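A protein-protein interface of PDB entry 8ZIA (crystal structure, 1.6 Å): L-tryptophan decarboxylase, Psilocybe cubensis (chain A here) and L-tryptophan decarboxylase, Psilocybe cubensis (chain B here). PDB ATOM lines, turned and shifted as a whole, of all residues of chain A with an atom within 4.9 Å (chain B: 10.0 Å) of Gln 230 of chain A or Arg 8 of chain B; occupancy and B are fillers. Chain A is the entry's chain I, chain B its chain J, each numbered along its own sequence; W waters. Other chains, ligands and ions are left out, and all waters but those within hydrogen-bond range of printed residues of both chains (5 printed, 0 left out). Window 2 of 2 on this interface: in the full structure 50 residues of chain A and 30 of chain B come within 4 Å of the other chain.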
ATOM      1  N   PHE A 227     -15.301 -15.030 -16.116  1.00  0.00           N
ATOM      2  CA  PHE A 227     -16.532 -14.700 -16.826  1.00  0.00           C
ATOM      3  C   PHE A 227     -16.613 -13.232 -17.218  1.00  0.00           C
ATOM      4  O   PHE A 227     -17.484 -12.867 -18.018  1.00  0.00           O
ATOM      5  CB  PHE A 227     -17.764 -15.031 -15.964  1.00  0.00           C
ATOM      6  CG  PHE A 227     -18.044 -16.506 -15.805  1.00  0.00           C
ATOM      7  CD1 PHE A 227     -17.781 -17.406 -16.820  1.00  0.00           C
ATOM      8  CD2 PHE A 227     -18.602 -16.983 -14.633  1.00  0.00           C
ATOM      9  CE1 PHE A 227     -18.056 -18.756 -16.662  1.00  0.00           C
ATOM     10  CE2 PHE A 227     -18.883 -18.334 -14.476  1.00  0.00           C
ATOM     11  CZ  PHE A 227     -18.610 -19.217 -15.487  1.00  0.00           C
ATOM     12  N   THR A 228     -15.741 -12.385 -16.676  1.00  0.00           N
ATOM     13  CA  THR A 228     -15.875 -10.941 -16.868  1.00  0.00           C
ATOM     14  C   THR A 228     -16.042 -10.537 -18.327  1.00  0.00           C
ATOM     15  O   THR A 228     -16.924  -9.712 -18.621  1.00  0.00           O
ATOM     16  CB  THR A 228     -14.662 -10.232 -16.252  1.00  0.00           C
ATOM     17  OG1 THR A 228     -14.589 -10.534 -14.854  1.00  0.00           O
ATOM     18  CG2 THR A 228     -14.771  -8.721 -16.433  1.00  0.00           C
ATOM     19  N   PRO A 229     -15.261 -11.059 -19.276  1.00  0.00           N
ATOM     20  CA  PRO A 229     -15.417 -10.608 -20.667  1.00  0.00           C
ATOM     21  C   PRO A 229     -16.812 -10.799 -21.224  1.00  0.00           C
ATOM     22  O   PRO A 229     -17.216 -10.039 -22.113  1.00  0.00           O
ATOM     23  CB  PRO A 229     -14.396 -11.461 -21.432  1.00  0.00           C
ATOM     24  CG  PRO A 229     -13.421 -11.894 -20.414  1.00  0.00           C
ATOM     25  CD  PRO A 229     -14.164 -12.025 -19.116  1.00  0.00           C
ATOM     26  N   GLN A 230     -17.558 -11.798 -20.747  1.00  0.00           N
ATOM     27  CA  GLN A 230     -18.899 -12.013 -21.273  1.00  0.00           C
ATOM     28  C   GLN A 230     -19.825 -10.847 -20.965  1.00  0.00           C
ATOM     29  O   GLN A 230     -20.866 -10.711 -21.615  1.00  0.00           O
ATOM     30  CB  GLN A 230     -19.491 -13.305 -20.716  1.00  0.00           C
ATOM     31  CG  GLN A 230     -18.675 -14.551 -21.009  1.00  0.00           C
ATOM     32  CD  GLN A 230     -19.457 -15.817 -20.758  1.00  0.00           C
ATOM     33  OE1 GLN A 230     -20.647 -15.889 -21.065  1.00  0.00           O
ATOM     34  NE2 GLN A 230     -18.803 -16.817 -20.175  1.00  0.00           N
ATOM     35  N   PHE A 231     -19.473 -10.007 -19.991  1.00  0.00           N
ATOM     36  CA  PHE A 231     -20.337  -8.914 -19.575  1.00  0.00           C
ATOM     37  C   PHE A 231     -19.894  -7.570 -20.107  1.00  0.00           C
ATOM     38  O   PHE A 231     -20.600  -6.577 -19.907  1.00  0.00           O
ATOM     39  CB  PHE A 231     -20.447  -8.896 -18.040  1.00  0.00           C
ATOM     40  CG  PHE A 231     -21.233 -10.059 -17.515  1.00  0.00           C
ATOM     41  CD1 PHE A 231     -22.606  -9.984 -17.416  1.00  0.00           C
ATOM     42  CD2 PHE A 231     -20.602 -11.262 -17.208  1.00  0.00           C
ATOM     43  CE1 PHE A 231     -23.339 -11.069 -16.976  1.00  0.00           C
ATOM     44  CE2 PHE A 231     -21.335 -12.348 -16.764  1.00  0.00           C
ATOM     45  CZ  PHE A 231     -22.706 -12.242 -16.643  1.00  0.00           C
ATOM     46  N   GLU A 232     -18.763  -7.510 -20.816  1.00  0.00           N
ATOM     47  CA  GLU A 232     -18.380  -6.269 -21.466  1.00  0.00           C
ATOM     48  C   GLU A 232     -19.470  -5.861 -22.451  1.00  0.00           C
ATOM     49  O   GLU A 232     -20.025  -6.702 -23.170  1.00  0.00           O
ATOM     50  CB  GLU A 232     -17.030  -6.441 -22.174  1.00  0.00           C
ATOM     51  CG  GLU A 232     -15.862  -6.808 -21.227  1.00  0.00           C
ATOM     52  CD  GLU A 232     -15.339  -5.614 -20.435  1.00  0.00           C
ATOM     53  OE1 GLU A 232     -15.775  -4.485 -20.744  1.00  0.00           O
ATOM     54  OE2 GLU A 232     -14.490  -5.797 -19.513  1.00  0.00           O
ATOM     55  N   GLY A 234     -22.360  -4.972 -21.510  1.00  0.00           N
ATOM     56  CA  GLY A 234     -23.639  -5.340 -20.930  1.00  0.00           C
ATOM     57  C   GLY A 234     -24.275  -4.200 -20.157  1.00  0.00           C
ATOM     58  O   GLY A 234     -23.908  -3.033 -20.296  1.00  0.00           O
ATOM     59  N   LYS A 312     -31.990 -19.659 -22.272  1.00  0.00           N
ATOM     60  CA  LYS A 312     -30.670 -19.260 -22.742  1.00  0.00           C
ATOM     61  C   LYS A 312     -30.686 -17.964 -23.548  1.00  0.00           C
ATOM     62  O   LYS A 312     -29.607 -17.436 -23.844  1.00  0.00           O
ATOM     63  CB  LYS A 312     -30.040 -20.396 -23.552  1.00  0.00           C
ATOM     64  CG  LYS A 312     -29.784 -21.654 -22.718  1.00  0.00           C
ATOM     65  CD  LYS A 312     -28.905 -21.352 -21.505  1.00  0.00           C
ATOM     66  CE  LYS A 312     -28.617 -22.610 -20.690  1.00  0.00           C
ATOM     67  NZ  LYS A 312     -29.806 -23.132 -19.958  1.00  0.00           N
ATOM     68  N   ILE A 314     -31.729 -15.486 -22.003  1.00  0.00           N
ATOM     69  CA  ILE A 314     -31.177 -14.728 -20.888  1.00  0.00           C
ATOM     70  C   ILE A 314     -29.776 -15.207 -20.554  1.00  0.00           C
ATOM     71  O   ILE A 314     -28.842 -14.409 -20.429  1.00  0.00           O
ATOM     72  CB  ILE A 314     -32.101 -14.840 -19.662  1.00  0.00           C
ATOM     73  CG1 ILE A 314     -33.385 -14.066 -19.899  1.00  0.00           C
ATOM     74  CG2 ILE A 314     -31.372 -14.348 -18.400  1.00  0.00           C
ATOM     75  CD1 ILE A 314     -34.442 -14.376 -18.854  1.00  0.00           C
ATOM     76  N   GLY A 315     -29.621 -16.525 -20.421  1.00  0.00           N
ATOM     77  CA  GLY A 315     -28.301 -17.113 -20.265  1.00  0.00           C
ATOM     78  C   GLY A 315     -27.628 -16.698 -18.971  1.00  0.00           C
ATOM     79  O   GLY A 315     -28.267 -16.543 -17.926  1.00  0.00           O
ATOM     80  N   LEU A 316     -26.315 -16.520 -19.045  1.00  0.00           N
ATOM     81  CA  LEU A 316     -25.521 -16.228 -17.861  1.00  0.00           C
ATOM     82  C   LEU A 316     -25.755 -14.793 -17.411  1.00  0.00           C
ATOM     83  O   LEU A 316     -25.649 -13.854 -18.205  1.00  0.00           O
ATOM     84  CB  LEU A 316     -24.035 -16.461 -18.161  1.00  0.00           C
ATOM     85  CG  LEU A 316     -23.114 -16.339 -16.958  1.00  0.00           C
ATOM     86  CD1 LEU A 316     -23.331 -17.494 -15.987  1.00  0.00           C
ATOM     87  CD2 LEU A 316     -21.647 -16.267 -17.413  1.00  0.00           C
ATOM     88  N   LEU B   5     -27.512  -6.278 -10.499  1.00  0.00           N
ATOM     89  CA  LEU B   5     -27.866  -7.310 -11.462  1.00  0.00           C
ATOM     90  C   LEU B   5     -27.150  -6.983 -12.757  1.00  0.00           C
ATOM     91  O   LEU B   5     -27.281  -5.868 -13.263  1.00  0.00           O
ATOM     92  CB  LEU B   5     -29.382  -7.345 -11.684  1.00  0.00           C
ATOM     93  CG  LEU B   5     -29.899  -8.134 -12.891  1.00  0.00           C
ATOM     94  CD1 LEU B   5     -29.712  -9.633 -12.668  1.00  0.00           C
ATOM     95  CD2 LEU B   5     -31.366  -7.798 -13.219  1.00  0.00           C
ATOM     96  N   GLY B   6     -26.395  -7.945 -13.273  1.00  0.00           N
ATOM     97  CA  GLY B   6     -25.638  -7.744 -14.500  1.00  0.00           C
ATOM     98  C   GLY B   6     -26.147  -8.626 -15.621  1.00  0.00           C
ATOM     99  O   GLY B   6     -26.293  -9.843 -15.450  1.00  0.00           O
ATOM    100  N   LEU B   7     -26.379  -8.018 -16.785  1.00  0.00           N
ATOM    101  CA  LEU B   7     -26.872  -8.699 -17.974  1.00  0.00           C
ATOM    102  C   LEU B   7     -25.860  -8.551 -19.100  1.00  0.00           C
ATOM    103  O   LEU B   7     -25.270  -7.482 -19.276  1.00  0.00           O
ATOM    104  CB  LEU B   7     -28.211  -8.117 -18.421  1.00  0.00           C
ATOM    105  CG  LEU B   7     -29.247  -8.063 -17.299  1.00  0.00           C
ATOM    106  CD1 LEU B   7     -30.550  -7.400 -17.783  1.00  0.00           C
ATOM    107  CD2 LEU B   7     -29.503  -9.471 -16.785  1.00  0.00           C
ATOM    108  N   ARG B   8     -25.668  -9.629 -19.852  1.00  0.00           N
ATOM    109  CA  ARG B   8     -24.792  -9.585 -21.015  1.00  0.00           C
ATOM    110  C   ARG B   8     -25.462  -8.797 -22.140  1.00  0.00           C
ATOM    111  O   ARG B   8     -26.688  -8.669 -22.201  1.00  0.00           O
ATOM    112  CB  ARG B   8     -24.445 -11.005 -21.472  1.00  0.00           C
ATOM    113  CG  ARG B   8     -23.694 -11.827 -20.423  1.00  0.00           C
ATOM    114  CD  ARG B   8     -23.530 -13.291 -20.813  1.00  0.00           C
ATOM    115  NE  ARG B   8     -24.823 -13.933 -21.003  1.00  0.00           N
ATOM    116  CZ  ARG B   8     -25.336 -14.266 -22.181  1.00  0.00           C
ATOM    117  NH1 ARG B   8     -24.625 -14.190 -23.296  1.00  0.00           N
ATOM    118  NH2 ARG B   8     -26.598 -14.676 -22.243  1.00  0.00           N
ATOM    119  N   LYS B   9     -24.637  -8.268 -23.049  1.00  0.00           N
ATOM    120  CA  LYS B   9     -25.182  -7.470 -24.145  1.00  0.00           C
ATOM    121  C   LYS B   9     -26.183  -8.266 -24.978  1.00  0.00           C
ATOM    122  O   LYS B   9     -27.211  -7.729 -25.410  1.00  0.00           O
ATOM    123  CB  LYS B   9     -24.045  -6.945 -25.018  1.00  0.00           C
ATOM    124  CG  LYS B   9     -24.525  -6.250 -26.285  1.00  0.00           C
ATOM    125  CD  LYS B   9     -23.610  -5.104 -26.667  1.00  0.00           C
ATOM    126  CE  LYS B   9     -23.470  -4.976 -28.176  1.00  0.00           C
ATOM    127  NZ  LYS B   9     -22.192  -5.578 -28.657  1.00  0.00           N
ATOM    128  N   ASP B  10     -25.910  -9.555 -25.193  1.00  0.00           N
ATOM    129  CA  ASP B  10     -26.796 -10.420 -25.968  1.00  0.00           C
ATOM    130  C   ASP B  10     -28.039 -10.865 -25.205  1.00  0.00           C
ATOM    131  O   ASP B  10     -28.954 -11.429 -25.820  1.00  0.00           O
ATOM    132  CB  ASP B  10     -26.024 -11.650 -26.452  1.00  0.00           C
ATOM    133  CG  ASP B  10     -25.075 -11.326 -27.592  1.00  0.00           C
ATOM    134  OD1 ASP B  10     -25.135 -10.189 -28.112  1.00  0.00           O
ATOM    135  OD2 ASP B  10     -24.275 -12.207 -27.975  1.00  0.00           O
ATOM    136  N   CYS B  11     -28.103 -10.634 -23.898  1.00  0.00           N
ATOM    137  CA  CYS B  11     -29.309 -10.954 -23.145  1.00  0.00           C
ATOM    138  C   CYS B  11     -30.505 -10.251 -23.772  1.00  0.00           C
ATOM    139  O   CYS B  11     -30.502  -9.028 -23.942  1.00  0.00           O
ATOM    140  CB  CYS B  11     -29.147 -10.523 -21.691  1.00  0.00           C
ATOM    141  SG  CYS B  11     -30.461 -10.997 -20.568  1.00  0.00           S
ATOM    142  N   ARG B  12     -31.529 -11.025 -24.128  1.00  0.00           N
ATOM    143  CA  ARG B  12     -32.709 -10.418 -24.727  1.00  0.00           C
ATOM    144  C   ARG B  12     -33.609  -9.743 -23.703  1.00  0.00           C
ATOM    145  O   ARG B  12     -34.438  -8.909 -24.083  1.00  0.00           O
ATOM    146  CB  ARG B  12     -33.509 -11.461 -25.510  1.00  0.00           C
ATOM    147  CG  ARG B  12     -33.021 -11.671 -26.935  1.00  0.00           C
ATOM    148  CD  ARG B  12     -31.902 -12.694 -26.994  1.00  0.00           C
ATOM    149  NE  ARG B  12     -31.839 -13.330 -28.306  1.00  0.00           N
ATOM    150  CZ  ARG B  12     -31.350 -14.544 -28.531  1.00  0.00           C
ATOM    151  NH1 ARG B  12     -30.881 -15.295 -27.546  1.00  0.00           N
ATOM    152  NH2 ARG B  12     -31.334 -15.018 -29.775  1.00  0.00           N
ATOM    153  N   ALA B  13     -33.473 -10.083 -22.423  1.00  0.00           N
ATOM    154  CA  ALA B  13     -34.186  -9.365 -21.378  1.00  0.00           C
ATOM    155  C   ALA B  13     -33.511  -8.024 -21.141  1.00  0.00           C
ATOM    156  O   ALA B  13     -32.301  -7.959 -20.899  1.00  0.00           O
ATOM    157  CB  ALA B  13     -34.227 -10.178 -20.083  1.00  0.00           C
ATOM    158  N   GLU B  14     -34.290  -6.954 -21.231  1.00  0.00           N
ATOM    159  CA  GLU B  14     -33.808  -5.597 -21.044  1.00  0.00           C
ATOM    160  C   GLU B  14     -34.390  -5.025 -19.762  1.00  0.00           C
ATOM    161  O   GLU B  14     -35.545  -5.299 -19.418  1.00  0.00           O
ATOM    162  CB  GLU B  14     -34.197  -4.703 -22.220  1.00  0.00           C
ATOM    163  CG  GLU B  14     -33.520  -5.058 -23.522  1.00  0.00           C
ATOM    164  CD  GLU B  14     -34.029  -4.212 -24.674  1.00  0.00           C
ATOM    165  OE1 GLU B  14     -35.015  -3.467 -24.475  1.00  0.00           O
ATOM    166  OE2 GLU B  14     -33.444  -4.287 -25.775  1.00  0.00           O
ATOM    167  N   ILE B  15     -33.588  -4.209 -19.078  1.00  0.00           N
ATOM    168  CA  ILE B  15     -34.014  -3.607 -17.820  1.00  0.00           C
ATOM    169  C   ILE B  15     -35.273  -2.771 -18.026  1.00  0.00           C
ATOM    170  O   ILE B  15     -35.397  -2.009 -18.997  1.00  0.00           O
ATOM    171  CB  ILE B  15     -32.861  -2.779 -17.230  1.00  0.00           C
ATOM    172  CG1 ILE B  15     -31.705  -3.711 -16.863  1.00  0.00           C
ATOM    173  CG2 ILE B  15     -33.317  -2.006 -15.995  1.00  0.00           C
ATOM    174  CD1 ILE B  15     -30.384  -2.999 -16.656  1.00  0.00           C
ATOM    175  N   ALA B  33     -36.432  -7.001 -15.480  1.00  0.00           N
ATOM    176  CA  ALA B  33     -35.954  -7.125 -16.851  1.00  0.00           C
ATOM    177  C   ALA B  33     -36.805  -8.167 -17.559  1.00  0.00           C
ATOM    178  O   ALA B  33     -37.259  -9.135 -16.943  1.00  0.00           O
ATOM    179  CB  ALA B  33     -34.468  -7.505 -16.897  1.00  0.00           C
HETATM  180  O   HOH W   1     -21.962  -8.600 -22.784  1.00  0.00           O
HETATM  181  O   HOH W   2     -27.264 -12.042 -19.444  1.00  0.00           O
HETATM  182  O   HOH W   3     -21.677 -14.843 -23.320  1.00  0.00           O
HETATM  183  O   HOH W   4     -28.088 -15.212 -24.583  1.00  0.00           O
HETATM  184  O   HOH W   5     -25.043 -17.594 -21.471  1.00  0.00           O
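The side-chain sulfur of Cys 11 of chain B sits at hydrogen-bond distance from the backbone carbonyl oxygen of Ile 314 of chain A (3.8 Å). The backbone carbonyl oxygen (O) of Leu 316 of chain A lies within hydrogen-bond range of the guanidinium group (NE) of Arg 8 of chain B (2.9 Å). The backbone carbonyl oxygen (O) of Ile 314 of chain A sits at hydrogen-bond distance from the guanidinium group (NH2) of Arg 8 of chain B (2.9 Å).
SG of Cys 11 of chain B sits at hydrogen-bond distance from O of Ala 13 of chain B.
Among the printed residues, pairs that only touch across the chains: Gly 234 of chain A with Leu 7 of chain B (3.2 Å), Gln 230 of chain A with Arg 8 of chain B (3.3 Å), Phe 231 of chain A with Gly 6 of chain B (3.5 Å), Phe 231 of chain A with Arg 8 of chain B (3.5 Å), Gly 315 of chain A with Arg 8 of chain B (3.6 Å), Gly 234 of chain A with Lys 9 of chain B (3.7 Å), Phe 231 of chain A with Leu 7 of chain B (3.9 Å) and Ile 314 of chain A with Ala 13 of chain B (3.98 Å).
Arg 8 of chain B touches five residues of chain A. No residue of chain B comes within 4 Å of Phe 227 of chain A. No residue of chain B comes within 4 Å of Pro 229 of chain A. Of chain B, only Gly 6 (3.5 Å), Leu 7 (3.9 Å) and Arg 8 (3.5 Å) come within 4 Å of Phe 231 of chain A. Gly 315 of chain A touches one residue of chain B. Printed residues of chain A within 4 Å of Gly 6 of chain B: Phe 231 (3.5 Å). Of the printed residues of chain A, Ala 13 of chain B touches Ile 314 (3.98 Å). Leu 5 of chain B touches none of the printed residues of chain A. The nearest residue of chain A that does not touch Arg 8 of chain B is Gly 234 of chain A (4.1 Å).
Of the 11 printed residues of chain A, 6 touch a printed residue of chain B. Hydrophobic or aromatic side chains of chain A within 4 Å of the printed part of chain B: Phe 231, Ile 314 and Leu 316. Printed residues of chain B that touch a printed residue of chain A: Gly 6, Leu 7, Arg 8, Lys 9, Cys 11 and Ala 13. Hydrophobic or aromatic side chains of chain B that line the printed part of chain A: Ala 13. Among the printed residues, no Asp or Glu carboxylate lies within 4 Å of a Lys or Arg side-chain nitrogen of the other chain.
Water W1 lies within hydrogen-bond range of the backbone carbonyl oxygen (O) of Gln 230 of chain A (2.7 Å), the backbone NH (N) of Lys 9 of chain B (2.7 Å) and the backbone carbonyl oxygen (O) of Glu 232 of chain A (2.7 Å). Water W3 bridges OE1 of Gln 230 of chain A (2.7 Å) and NH1 of Arg 8 of chain B (3.0 Å). Water W2 lies within hydrogen-bond range of the backbone carbonyl oxygen (O) of Leu 316 of chain A, the backbone NH (N) of Arg 8 of chain B, the backbone carbonyl oxygen (O) of Ile 314 of chain A and the side-chain sulfur (SG) of Cys 11 of chain B. Water W4 bridges the backbone carbonyl oxygen (O) of Lys 312 of chain A (2.8 Å) and the guanidinium group (NH2) of Arg 8 of chain B (2.8 Å). Water W5 lies within hydrogen-bond range of N of Leu 316 of chain A and NH2 of Arg 8 of chain B.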
